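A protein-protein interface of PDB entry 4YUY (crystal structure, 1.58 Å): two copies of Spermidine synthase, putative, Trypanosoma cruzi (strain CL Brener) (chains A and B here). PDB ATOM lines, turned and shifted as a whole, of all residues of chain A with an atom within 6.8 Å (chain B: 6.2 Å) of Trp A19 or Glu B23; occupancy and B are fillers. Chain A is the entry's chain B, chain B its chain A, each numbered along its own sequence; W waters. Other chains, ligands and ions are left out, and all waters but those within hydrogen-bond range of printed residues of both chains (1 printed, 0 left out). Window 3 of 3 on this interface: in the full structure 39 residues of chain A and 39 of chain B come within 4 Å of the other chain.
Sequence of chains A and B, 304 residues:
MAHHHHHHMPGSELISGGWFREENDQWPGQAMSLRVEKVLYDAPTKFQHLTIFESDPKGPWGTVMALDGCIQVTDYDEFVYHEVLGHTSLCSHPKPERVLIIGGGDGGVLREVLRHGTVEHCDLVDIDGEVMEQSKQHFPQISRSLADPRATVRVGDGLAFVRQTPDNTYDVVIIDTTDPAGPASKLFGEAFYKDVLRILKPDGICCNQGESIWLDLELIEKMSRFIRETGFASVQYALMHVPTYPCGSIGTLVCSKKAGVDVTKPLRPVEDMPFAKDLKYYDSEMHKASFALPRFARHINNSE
The backbone NH (N) of Arg A35 is in hydrogen-bond range of the backbone carbonyl oxygen (O) of Gly B29 (2.8 Å).
O of Ala B31 lies within hydrogen-bond range of OG of Ser A33 (2.6 Å).
The backbone NH (N) of Arg B21 sits at hydrogen-bond distance from the backbone carbonyl oxygen (O) of Leu B14, at 2.9 Å.
The backbone carbonyl oxygen (O) of Leu A14 sits at hydrogen-bond distance from the backbone NH (N) of Arg A21 (3.0 Å).
The backbone carbonyl oxygen of Gly A18 lies within hydrogen-bond range of the guanidinium group of Arg A35 (2.9 Å).
The backbone NH (N) of Phe A20 is in hydrogen-bond range of the backbone carbonyl oxygen (O) of Leu A34 (2.9 Å).
N of Asp A56 is in hydrogen-bond range of O of Arg A35, at 3.4 Å.
OE1 of Glu B23 touches CZ2 of Trp A19, at 3.98 Å.
CZ3 of Trp A19 touches O of Gly B29, 3.9 Å away.
CZ3 of Trp A19 touches C of Gln B30, at 3.8 Å.
Ala B31 touches Trp A19 (N to CZ3, 3.9 Å).
NH1 of Arg B21 touches CD of Arg A21, 3.7 Å away.
Gln B30 touches Ser A33.
Leu A34 touches Gly B29.
Gln B30 touches Leu A34 (CB to CD2, 3.8 Å).
Gly B29 touches Asp A56.
Trp A19 touches just these residues of chain B: Glu B23 (3.98 Å), Gly B29 (3.9 Å), Gln B30 (3.8 Å) and Ala B31 (3.9 Å).
Of the printed residues of chain B, Leu A34 touches Gly B29 (3.4 Å) and Gln B30 (3.8 Å).
Printed residues of chain B within 4 Å of Arg A21: Arg B21 (3.7 Å).
Of the printed residues of chain A, Gly B29 touches Trp A19, Leu A34, Arg A35 and Asp A56.
Of the printed residues of chain B, Arg A35 touches Gly B29.
Val A36 touches none of the printed residues of chain B.
Trp B27 touches none of the printed residues of chain A.
The nearest printed residue of chain B that does not touch Trp A19 is Trp B27 (6.5 Å).
The nearest residue of chain A that does not touch Glu B23 is Ser A33 (6.2 Å).
Of the 14 printed residues of chain B, 5 touch a printed residue of chain A.
Hydrophobic or aromatic side chains of chain B within 4 Å of the printed part of chain A: Ala B31.
Among the printed residues, no Asp or Glu carboxylate lies within 4 Å of a Lys or Arg side-chain nitrogen of the other chain.
Arg A21 touches its own counterpart, Arg B21.
Water W1 lies within hydrogen-bond range of the backbone carbonyl oxygen of Gly B29, the backbone NH of Asp A56 and the backbone carbonyl oxygen of Arg A35.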
ATOM      1  N   GLU A  13      14.756  14.596  29.760  1.00  0.00           N
ATOM      2  CA  GLU A  13      13.953  15.716  29.312  1.00  0.00           C
ATOM      3  C   GLU A  13      12.453  15.386  28.976  1.00  0.00           C
ATOM      4  O   GLU A  13      11.599  16.287  28.976  1.00  0.00           O
ATOM      5  CB  GLU A  13      14.667  16.425  28.149  1.00  0.00           C
ATOM      6  CG  GLU A  13      14.631  15.683  26.804  1.00  0.00           C
ATOM      7  CD  GLU A  13      15.624  14.512  26.693  1.00  0.00           C
ATOM      8  OE1 GLU A  13      16.408  14.258  27.625  1.00  0.00           O
ATOM      9  OE2 GLU A  13      15.626  13.845  25.636  1.00  0.00           O
ATOM     10  N   LEU A  14      12.112  14.098  28.747  1.00  0.00           N
ATOM     11  CA  LEU A  14      10.724  13.764  28.496  1.00  0.00           C
ATOM     12  C   LEU A  14       9.721  13.997  29.630  1.00  0.00           C
ATOM     13  O   LEU A  14       8.473  14.058  29.387  1.00  0.00           O
ATOM     14  CB  LEU A  14      10.557  12.317  27.947  1.00  0.00           C
ATOM     15  CG  LEU A  14      11.146  12.061  26.580  1.00  0.00           C
ATOM     16  CD1 LEU A  14      10.600  10.666  26.230  1.00  0.00           C
ATOM     17  CD2 LEU A  14      10.799  13.125  25.532  1.00  0.00           C
ATOM     18  N   ILE A  15      10.229  14.153  30.857  1.00  0.00           N
ATOM     19  CA  ILE A  15       9.429  14.546  31.979  1.00  0.00           C
ATOM     20  C   ILE A  15       9.714  16.031  32.200  1.00  0.00           C
ATOM     21  O   ILE A  15      10.843  16.445  32.434  1.00  0.00           O
ATOM     22  CB  ILE A  15       9.787  13.749  33.261  1.00  0.00           C
ATOM     23  CG1 ILE A  15       9.454  12.255  33.077  1.00  0.00           C
ATOM     24  CG2 ILE A  15       9.043  14.342  34.459  1.00  0.00           C
ATOM     25  CD1 ILE A  15       9.698  11.403  34.325  1.00  0.00           C
ATOM     26  N   SER A  16       8.686  16.826  32.008  1.00  0.00           N
ATOM     27  CA  SER A  16       8.809  18.222  32.241  1.00  0.00           C
ATOM     28  C   SER A  16       7.406  18.719  32.417  1.00  0.00           C
ATOM     29  O   SER A  16       6.458  18.262  31.737  1.00  0.00           O
ATOM     30  CB  SER A  16       9.504  18.929  31.094  1.00  0.00           C
ATOM     31  OG  SER A  16       9.459  20.331  31.330  1.00  0.00           O
ATOM     32  N   GLY A  17       7.305  19.657  33.351  1.00  0.00           N
ATOM     33  CA  GLY A  17       6.057  20.307  33.703  1.00  0.00           C
ATOM     34  C   GLY A  17       4.957  19.424  34.227  1.00  0.00           C
ATOM     35  O   GLY A  17       3.807  19.757  33.973  1.00  0.00           O
ATOM     36  N   GLY A  18       5.281  18.319  34.946  1.00  0.00           N
ATOM     37  CA  GLY A  18       4.316  17.453  35.581  1.00  0.00           C
ATOM     38  C   GLY A  18       3.890  16.225  34.722  1.00  0.00           C
ATOM     39  O   GLY A  18       3.065  15.468  35.141  1.00  0.00           O
ATOM     40  N   TRP A  19       4.387  16.164  33.491  1.00  0.00           N
ATOM     41  CA  TRP A  19       3.945  15.104  32.533  1.00  0.00           C
ATOM     42  C   TRP A  19       5.129  14.409  31.928  1.00  0.00           C
ATOM     43  O   TRP A  19       6.191  14.978  31.697  1.00  0.00           O
ATOM     44  CB  TRP A  19       3.107  15.677  31.375  1.00  0.00           C
ATOM     45  CG  TRP A  19       1.692  16.181  31.782  1.00  0.00           C
ATOM     46  CD1 TRP A  19       1.370  17.382  32.409  1.00  0.00           C
ATOM     47  CD2 TRP A  19       0.469  15.524  31.532  1.00  0.00           C
ATOM     48  NE1 TRP A  19       0.003  17.446  32.634  1.00  0.00           N
ATOM     49  CE2 TRP A  19      -0.575  16.329  32.058  1.00  0.00           C
ATOM     50  CE3 TRP A  19       0.134  14.293  30.944  1.00  0.00           C
ATOM     51  CZ2 TRP A  19      -1.921  15.941  32.005  1.00  0.00           C
ATOM     52  CZ3 TRP A  19      -1.253  13.943  30.860  1.00  0.00           C
ATOM     53  CH2 TRP A  19      -2.247  14.747  31.386  1.00  0.00           C
ATOM     54  N   PHE A  20       4.887  13.145  31.510  1.00  0.00           N
ATOM     55  CA  PHE A  20       5.798  12.398  30.708  1.00  0.00           C
ATOM     56  C   PHE A  20       5.156  12.354  29.346  1.00  0.00           C
ATOM     57  O   PHE A  20       3.989  11.938  29.231  1.00  0.00           O
ATOM     58  CB  PHE A  20       5.964  10.959  31.264  1.00  0.00           C
ATOM     59  CG  PHE A  20       6.758  10.034  30.353  1.00  0.00           C
ATOM     60  CD1 PHE A  20       6.127   9.271  29.365  1.00  0.00           C
ATOM     61  CD2 PHE A  20       8.149   9.915  30.499  1.00  0.00           C
ATOM     62  CE1 PHE A  20       6.901   8.456  28.527  1.00  0.00           C
ATOM     63  CE2 PHE A  20       8.913   9.121  29.653  1.00  0.00           C
ATOM     64  CZ  PHE A  20       8.275   8.362  28.669  1.00  0.00           C
ATOM     65  N   ARG A  21       5.916  12.815  28.368  1.00  0.00           N
ATOM     66  CA  ARG A  21       5.544  12.858  26.966  1.00  0.00           C
ATOM     67  C   ARG A  21       6.432  11.934  26.138  1.00  0.00           C
ATOM     68  O   ARG A  21       7.611  12.127  25.966  1.00  0.00           O
ATOM     69  CB  ARG A  21       5.662  14.338  26.499  1.00  0.00           C
ATOM     70  CG  ARG A  21       4.500  15.212  27.067  1.00  0.00           C
ATOM     71  CD  ARG A  21       4.435  16.668  26.491  1.00  0.00           C
ATOM     72  NE  ARG A  21       4.655  16.642  25.024  1.00  0.00           N
ATOM     73  CZ  ARG A  21       3.717  16.243  24.158  1.00  0.00           C
ATOM     74  NH1 ARG A  21       3.989  16.204  22.875  1.00  0.00           N
ATOM     75  NH2 ARG A  21       2.478  15.978  24.592  1.00  0.00           N
ATOM     76  N   SER A  33       0.926  10.793  26.466  1.00  0.00           N
ATOM     77  CA  SER A  33       1.458  11.407  27.658  1.00  0.00           C
ATOM     78  C   SER A  33       0.687  10.954  28.912  1.00  0.00           C
ATOM     79  O   SER A  33      -0.520  10.687  28.885  1.00  0.00           O
ATOM     80  CB  SER A  33       1.530  12.948  27.452  1.00  0.00           C
ATOM     81  OG  SER A  33       0.189  13.418  27.351  1.00  0.00           O
ATOM     82  N   LEU A  34       1.409  10.855  30.035  1.00  0.00           N
ATOM     83  CA  LEU A  34       0.891  10.440  31.307  1.00  0.00           C
ATOM     84  C   LEU A  34       1.316  11.426  32.364  1.00  0.00           C
ATOM     85  O   LEU A  34       2.439  11.828  32.358  1.00  0.00           O
ATOM     86  CB  LEU A  34       1.474   9.052  31.642  1.00  0.00           C
ATOM     87  CG  LEU A  34       0.841   7.912  30.795  1.00  0.00           C
ATOM     88  CD1 LEU A  34       1.633   6.653  31.098  1.00  0.00           C
ATOM     89  CD2 LEU A  34      -0.651   7.691  31.017  1.00  0.00           C
ATOM     90  N   ARG A  35       0.418  11.777  33.251  1.00  0.00           N
ATOM     91  CA  ARG A  35       0.783  12.744  34.326  1.00  0.00           C
ATOM     92  C   ARG A  35       1.756  12.005  35.252  1.00  0.00           C
ATOM     93  O   ARG A  35       1.598  10.794  35.509  1.00  0.00           O
ATOM     94  CB  ARG A  35      -0.472  13.100  35.116  1.00  0.00           C
ATOM     95  CG  ARG A  35      -0.403  14.426  35.845  1.00  0.00           C
ATOM     96  CD  ARG A  35      -1.662  15.251  35.597  1.00  0.00           C
ATOM     97  NE  ARG A  35      -1.431  16.692  35.834  1.00  0.00           N
ATOM     98  CZ  ARG A  35      -0.294  17.226  36.294  1.00  0.00           C
ATOM     99  NH1 ARG A  35       0.744  16.453  36.584  1.00  0.00           N
ATOM    100  NH2 ARG A  35      -0.189  18.538  36.486  1.00  0.00           N
ATOM    101  N   VAL A  36       2.722  12.741  35.785  1.00  0.00           N
ATOM    102  CA  VAL A  36       3.720  12.178  36.719  1.00  0.00           C
ATOM    103  C   VAL A  36       3.420  12.622  38.158  1.00  0.00           C
ATOM    104  O   VAL A  36       3.472  13.839  38.417  1.00  0.00           O
ATOM    105  CB  VAL A  36       5.114  12.641  36.341  1.00  0.00           C
ATOM    106  CG1 VAL A  36       6.155  12.174  37.360  1.00  0.00           C
ATOM    107  CG2 VAL A  36       5.487  12.187  34.914  1.00  0.00           C
ATOM    108  N   PHE A  53       8.267   5.913  37.075  1.00  0.00           N
ATOM    109  CA  PHE A  53       7.407   6.845  37.823  1.00  0.00           C
ATOM    110  C   PHE A  53       6.047   6.347  38.265  1.00  0.00           C
ATOM    111  O   PHE A  53       5.461   5.487  37.613  1.00  0.00           O
ATOM    112  CB  PHE A  53       7.286   8.194  37.023  1.00  0.00           C
ATOM    113  CG  PHE A  53       6.536   8.137  35.694  1.00  0.00           C
ATOM    114  CD1 PHE A  53       7.207   7.834  34.454  1.00  0.00           C
ATOM    115  CD2 PHE A  53       5.175   8.444  35.657  1.00  0.00           C
ATOM    116  CE1 PHE A  53       6.477   7.863  33.239  1.00  0.00           C
ATOM    117  CE2 PHE A  53       4.452   8.398  34.441  1.00  0.00           C
ATOM    118  CZ  PHE A  53       5.124   8.147  33.258  1.00  0.00           C
ATOM    119  N   ASP A  56      -0.473   9.549  37.832  1.00  0.00           N
ATOM    120  CA  ASP A  56      -1.589  10.177  38.564  1.00  0.00           C
ATOM    121  C   ASP A  56      -2.435   9.141  39.247  1.00  0.00           C
ATOM    122  O   ASP A  56      -3.013   8.303  38.575  1.00  0.00           O
ATOM    123  CB  ASP A  56      -2.418  10.936  37.552  1.00  0.00           C
ATOM    124  CG  ASP A  56      -3.341  11.964  38.163  1.00  0.00           C
ATOM    125  OD1 ASP A  56      -3.792  11.799  39.333  1.00  0.00           O
ATOM    126  OD2 ASP A  56      -3.668  12.906  37.404  1.00  0.00           O
ATOM    127  N   PRO B  10     -13.608  21.475  27.394  1.00  0.00           N
ATOM    128  CA  PRO B  10     -12.377  21.852  26.672  1.00  0.00           C
ATOM    129  C   PRO B  10     -12.619  22.574  25.331  1.00  0.00           C
ATOM    130  O   PRO B  10     -13.606  22.317  24.621  1.00  0.00           O
ATOM    131  CB  PRO B  10     -11.692  20.497  26.398  1.00  0.00           C
ATOM    132  CG  PRO B  10     -12.412  19.494  27.230  1.00  0.00           C
ATOM    133  CD  PRO B  10     -13.788  20.008  27.463  1.00  0.00           C
ATOM    134  N   LEU B  14      -6.481  23.465  24.394  1.00  0.00           N
ATOM    135  CA  LEU B  14      -5.822  22.232  24.118  1.00  0.00           C
ATOM    136  C   LEU B  14      -4.845  22.280  22.954  1.00  0.00           C
ATOM    137  O   LEU B  14      -4.113  21.357  22.811  1.00  0.00           O
ATOM    138  CB  LEU B  14      -6.872  21.065  23.966  1.00  0.00           C
ATOM    139  CG  LEU B  14      -7.903  20.881  25.107  1.00  0.00           C
ATOM    140  CD1 LEU B  14      -8.763  19.620  24.788  1.00  0.00           C
ATOM    141  CD2 LEU B  14      -7.150  20.716  26.419  1.00  0.00           C
ATOM    142  N   PHE B  20      -1.714  19.403  19.768  1.00  0.00           N
ATOM    143  CA  PHE B  20      -3.047  19.276  20.319  1.00  0.00           C
ATOM    144  C   PHE B  20      -2.932  18.210  21.405  1.00  0.00           C
ATOM    145  O   PHE B  20      -2.481  17.084  21.154  1.00  0.00           O
ATOM    146  CB  PHE B  20      -4.020  18.831  19.219  1.00  0.00           C
ATOM    147  CG  PHE B  20      -5.385  18.599  19.716  1.00  0.00           C
ATOM    148  CD1 PHE B  20      -5.745  17.340  20.257  1.00  0.00           C
ATOM    149  CD2 PHE B  20      -6.338  19.621  19.638  1.00  0.00           C
ATOM    150  CE1 PHE B  20      -7.025  17.166  20.704  1.00  0.00           C
ATOM    151  CE2 PHE B  20      -7.633  19.418  20.157  1.00  0.00           C
ATOM    152  CZ  PHE B  20      -7.955  18.169  20.656  1.00  0.00           C
ATOM    153  N   ARG B  21      -3.311  18.571  22.618  1.00  0.00           N
ATOM    154  CA  ARG B  21      -3.216  17.685  23.746  1.00  0.00           C
ATOM    155  C   ARG B  21      -4.588  17.335  24.301  1.00  0.00           C
ATOM    156  O   ARG B  21      -5.300  18.145  24.860  1.00  0.00           O
ATOM    157  CB  ARG B  21      -2.379  18.413  24.864  1.00  0.00           C
ATOM    158  CG  ARG B  21      -0.948  18.717  24.399  1.00  0.00           C
ATOM    159  CD  ARG B  21      -0.469  19.966  25.152  1.00  0.00           C
ATOM    160  NE  ARG B  21       0.598  20.650  24.424  1.00  0.00           N
ATOM    161  CZ  ARG B  21       1.894  20.436  24.656  1.00  0.00           C
ATOM    162  NH1 ARG B  21       2.259  19.575  25.610  1.00  0.00           N
ATOM    163  NH2 ARG B  21       2.820  21.120  23.981  1.00  0.00           N
ATOM    164  N   GLU B  22      -4.981  16.062  24.121  1.00  0.00           N
ATOM    165  CA  GLU B  22      -6.307  15.628  24.442  1.00  0.00           C
ATOM    166  C   GLU B  22      -6.519  15.340  25.939  1.00  0.00           C
ATOM    167  O   GLU B  22      -6.744  14.228  26.368  1.00  0.00           O
ATOM    168  CB  GLU B  22      -6.608  14.369  23.600  1.00  0.00           C
ATOM    169  CG  GLU B  22      -8.112  14.198  23.451  1.00  0.00           C
ATOM    170  CD  GLU B  22      -8.471  12.843  22.843  1.00  0.00           C
ATOM    171  OE1 GLU B  22      -7.790  11.849  23.154  1.00  0.00           O
ATOM    172  OE2 GLU B  22      -9.349  12.803  22.001  1.00  0.00           O
ATOM    173  N   GLU B  23      -6.375  16.377  26.779  1.00  0.00           N
ATOM    174  CA  GLU B  23      -6.608  16.240  28.182  1.00  0.00           C
ATOM    175  C   GLU B  23      -8.103  16.364  28.494  1.00  0.00           C
ATOM    176  O   GLU B  23      -8.765  17.284  27.979  1.00  0.00           O
ATOM    177  CB  GLU B  23      -5.857  17.386  28.922  1.00  0.00           C
ATOM    178  CG  GLU B  23      -4.327  17.400  28.775  1.00  0.00           C
ATOM    179  CD  GLU B  23      -3.690  18.621  29.423  1.00  0.00           C
ATOM    180  OE1 GLU B  23      -4.053  18.977  30.570  1.00  0.00           O
ATOM    181  OE2 GLU B  23      -2.836  19.232  28.773  1.00  0.00           O
ATOM    182  N   ASN B  24      -8.646  15.513  29.345  1.00  0.00           N
ATOM    183  CA  ASN B  24     -10.056  15.529  29.563  1.00  0.00           C
ATOM    184  C   ASN B  24     -10.337  14.856  30.856  1.00  0.00           C
ATOM    185  O   ASN B  24      -9.687  13.854  31.188  1.00  0.00           O
ATOM    186  CB  ASN B  24     -10.721  14.793  28.385  1.00  0.00           C
ATOM    187  CG  ASN B  24     -12.193  15.123  28.237  1.00  0.00           C
ATOM    188  OD1 ASN B  24     -13.034  14.611  29.021  1.00  0.00           O
ATOM    189  ND2 ASN B  24     -12.514  15.895  27.197  1.00  0.00           N
ATOM    190  N   ASP B  25     -11.308  15.363  31.603  1.00  0.00           N
ATOM    191  CA  ASP B  25     -11.600  14.646  32.827  1.00  0.00           C
ATOM    192  C   ASP B  25     -12.370  13.340  32.632  1.00  0.00           C
ATOM    193  O   ASP B  25     -12.634  12.640  33.572  1.00  0.00           O
ATOM    194  CB  ASP B  25     -12.138  15.573  33.936  1.00  0.00           C
ATOM    195  CG  ASP B  25     -13.349  16.303  33.522  1.00  0.00           C
ATOM    196  OD1 ASP B  25     -14.180  15.664  32.827  1.00  0.00           O
ATOM    197  OD2 ASP B  25     -13.470  17.511  33.903  1.00  0.00           O
ATOM    198  N   TRP B  27     -10.890  11.000  31.071  1.00  0.00           N
ATOM    199  CA  TRP B  27      -9.781  10.027  31.144  1.00  0.00           C
ATOM    200  C   TRP B  27      -8.659  10.748  31.900  1.00  0.00           C
ATOM    201  O   TRP B  27      -7.681  11.203  31.349  1.00  0.00           O
ATOM    202  CB  TRP B  27      -9.290   9.552  29.776  1.00  0.00           C
ATOM    203  CG  TRP B  27      -9.279  10.560  28.702  1.00  0.00           C
ATOM    204  CD1 TRP B  27      -8.295  11.471  28.414  1.00  0.00           C
ATOM    205  CD2 TRP B  27     -10.370  10.829  27.818  1.00  0.00           C
ATOM    206  NE1 TRP B  27      -8.687  12.238  27.293  1.00  0.00           N
ATOM    207  CE2 TRP B  27      -9.962  11.861  26.927  1.00  0.00           C
ATOM    208  CE3 TRP B  27     -11.573  10.196  27.610  1.00  0.00           C
ATOM    209  CZ2 TRP B  27     -10.804  12.352  25.909  1.00  0.00           C
ATOM    210  CZ3 TRP B  27     -12.421  10.644  26.617  1.00  0.00           C
ATOM    211  CH2 TRP B  27     -12.049  11.738  25.764  1.00  0.00           C
ATOM    212  N   GLY B  29      -5.491  11.818  34.053  1.00  0.00           N
ATOM    213  CA  GLY B  29      -4.051  11.428  34.078  1.00  0.00           C
ATOM    214  C   GLY B  29      -3.329  11.098  32.762  1.00  0.00           C
ATOM    215  O   GLY B  29      -2.142  10.718  32.780  1.00  0.00           O
ATOM    216  N   GLN B  30      -4.050  11.150  31.658  1.00  0.00           N
ATOM    217  CA  GLN B  30      -3.463  10.730  30.354  1.00  0.00           C
ATOM    218  C   GLN B  30      -3.913  11.693  29.285  1.00  0.00           C
ATOM    219  O   GLN B  30      -4.950  12.300  29.396  1.00  0.00           O
ATOM    220  CB  GLN B  30      -3.941   9.323  29.971  1.00  0.00           C
ATOM    221  CG  GLN B  30      -5.449   9.262  29.574  1.00  0.00           C
ATOM    222  CD  GLN B  30      -5.930   7.821  29.397  1.00  0.00           C
ATOM    223  OE1 GLN B  30      -6.087   7.318  28.220  1.00  0.00           O
ATOM    224  NE2 GLN B  30      -6.131   7.139  30.501  1.00  0.00           N
ATOM    225  N   ALA B  31      -3.156  11.745  28.199  1.00  0.00           N
ATOM    226  CA  ALA B  31      -3.497  12.563  27.035  1.00  0.00           C
ATOM    227  C   ALA B  31      -2.744  12.128  25.825  1.00  0.00           C
ATOM    228  O   ALA B  31      -1.494  12.131  25.765  1.00  0.00           O
ATOM    229  CB  ALA B  31      -3.175  14.064  27.294  1.00  0.00           C
ATOM    230  N   MET B  32      -3.517  11.703  24.844  1.00  0.00           N
ATOM    231  CA  MET B  32      -2.983  11.575  23.530  1.00  0.00           C
ATOM    232  C   MET B  32      -2.653  12.980  22.931  1.00  0.00           C
ATOM    233  O   MET B  32      -3.449  13.967  23.155  1.00  0.00           O
ATOM    234  CB  MET B  32      -3.891  10.670  22.631  1.00  0.00           C
ATOM    235  CG  MET B  32      -3.376  10.498  21.200  1.00  0.00           C
ATOM    236  SD  MET B  32      -1.753   9.761  21.250  1.00  0.00           S
ATOM    237  CE  MET B  32      -1.390   9.501  19.540  1.00  0.00           C
ATOM    238  N   GLY B  69     -12.749  19.202  22.608  1.00  0.00           N
ATOM    239  CA  GLY B  69     -11.441  18.724  22.967  1.00  0.00           C
ATOM    240  C   GLY B  69     -11.173  17.266  22.705  1.00  0.00           C
ATOM    241  O   GLY B  69     -10.088  16.789  23.009  1.00  0.00           O
HETATM  242  O   HOH W   1      -1.244   9.242  35.015  1.00  0.00           O
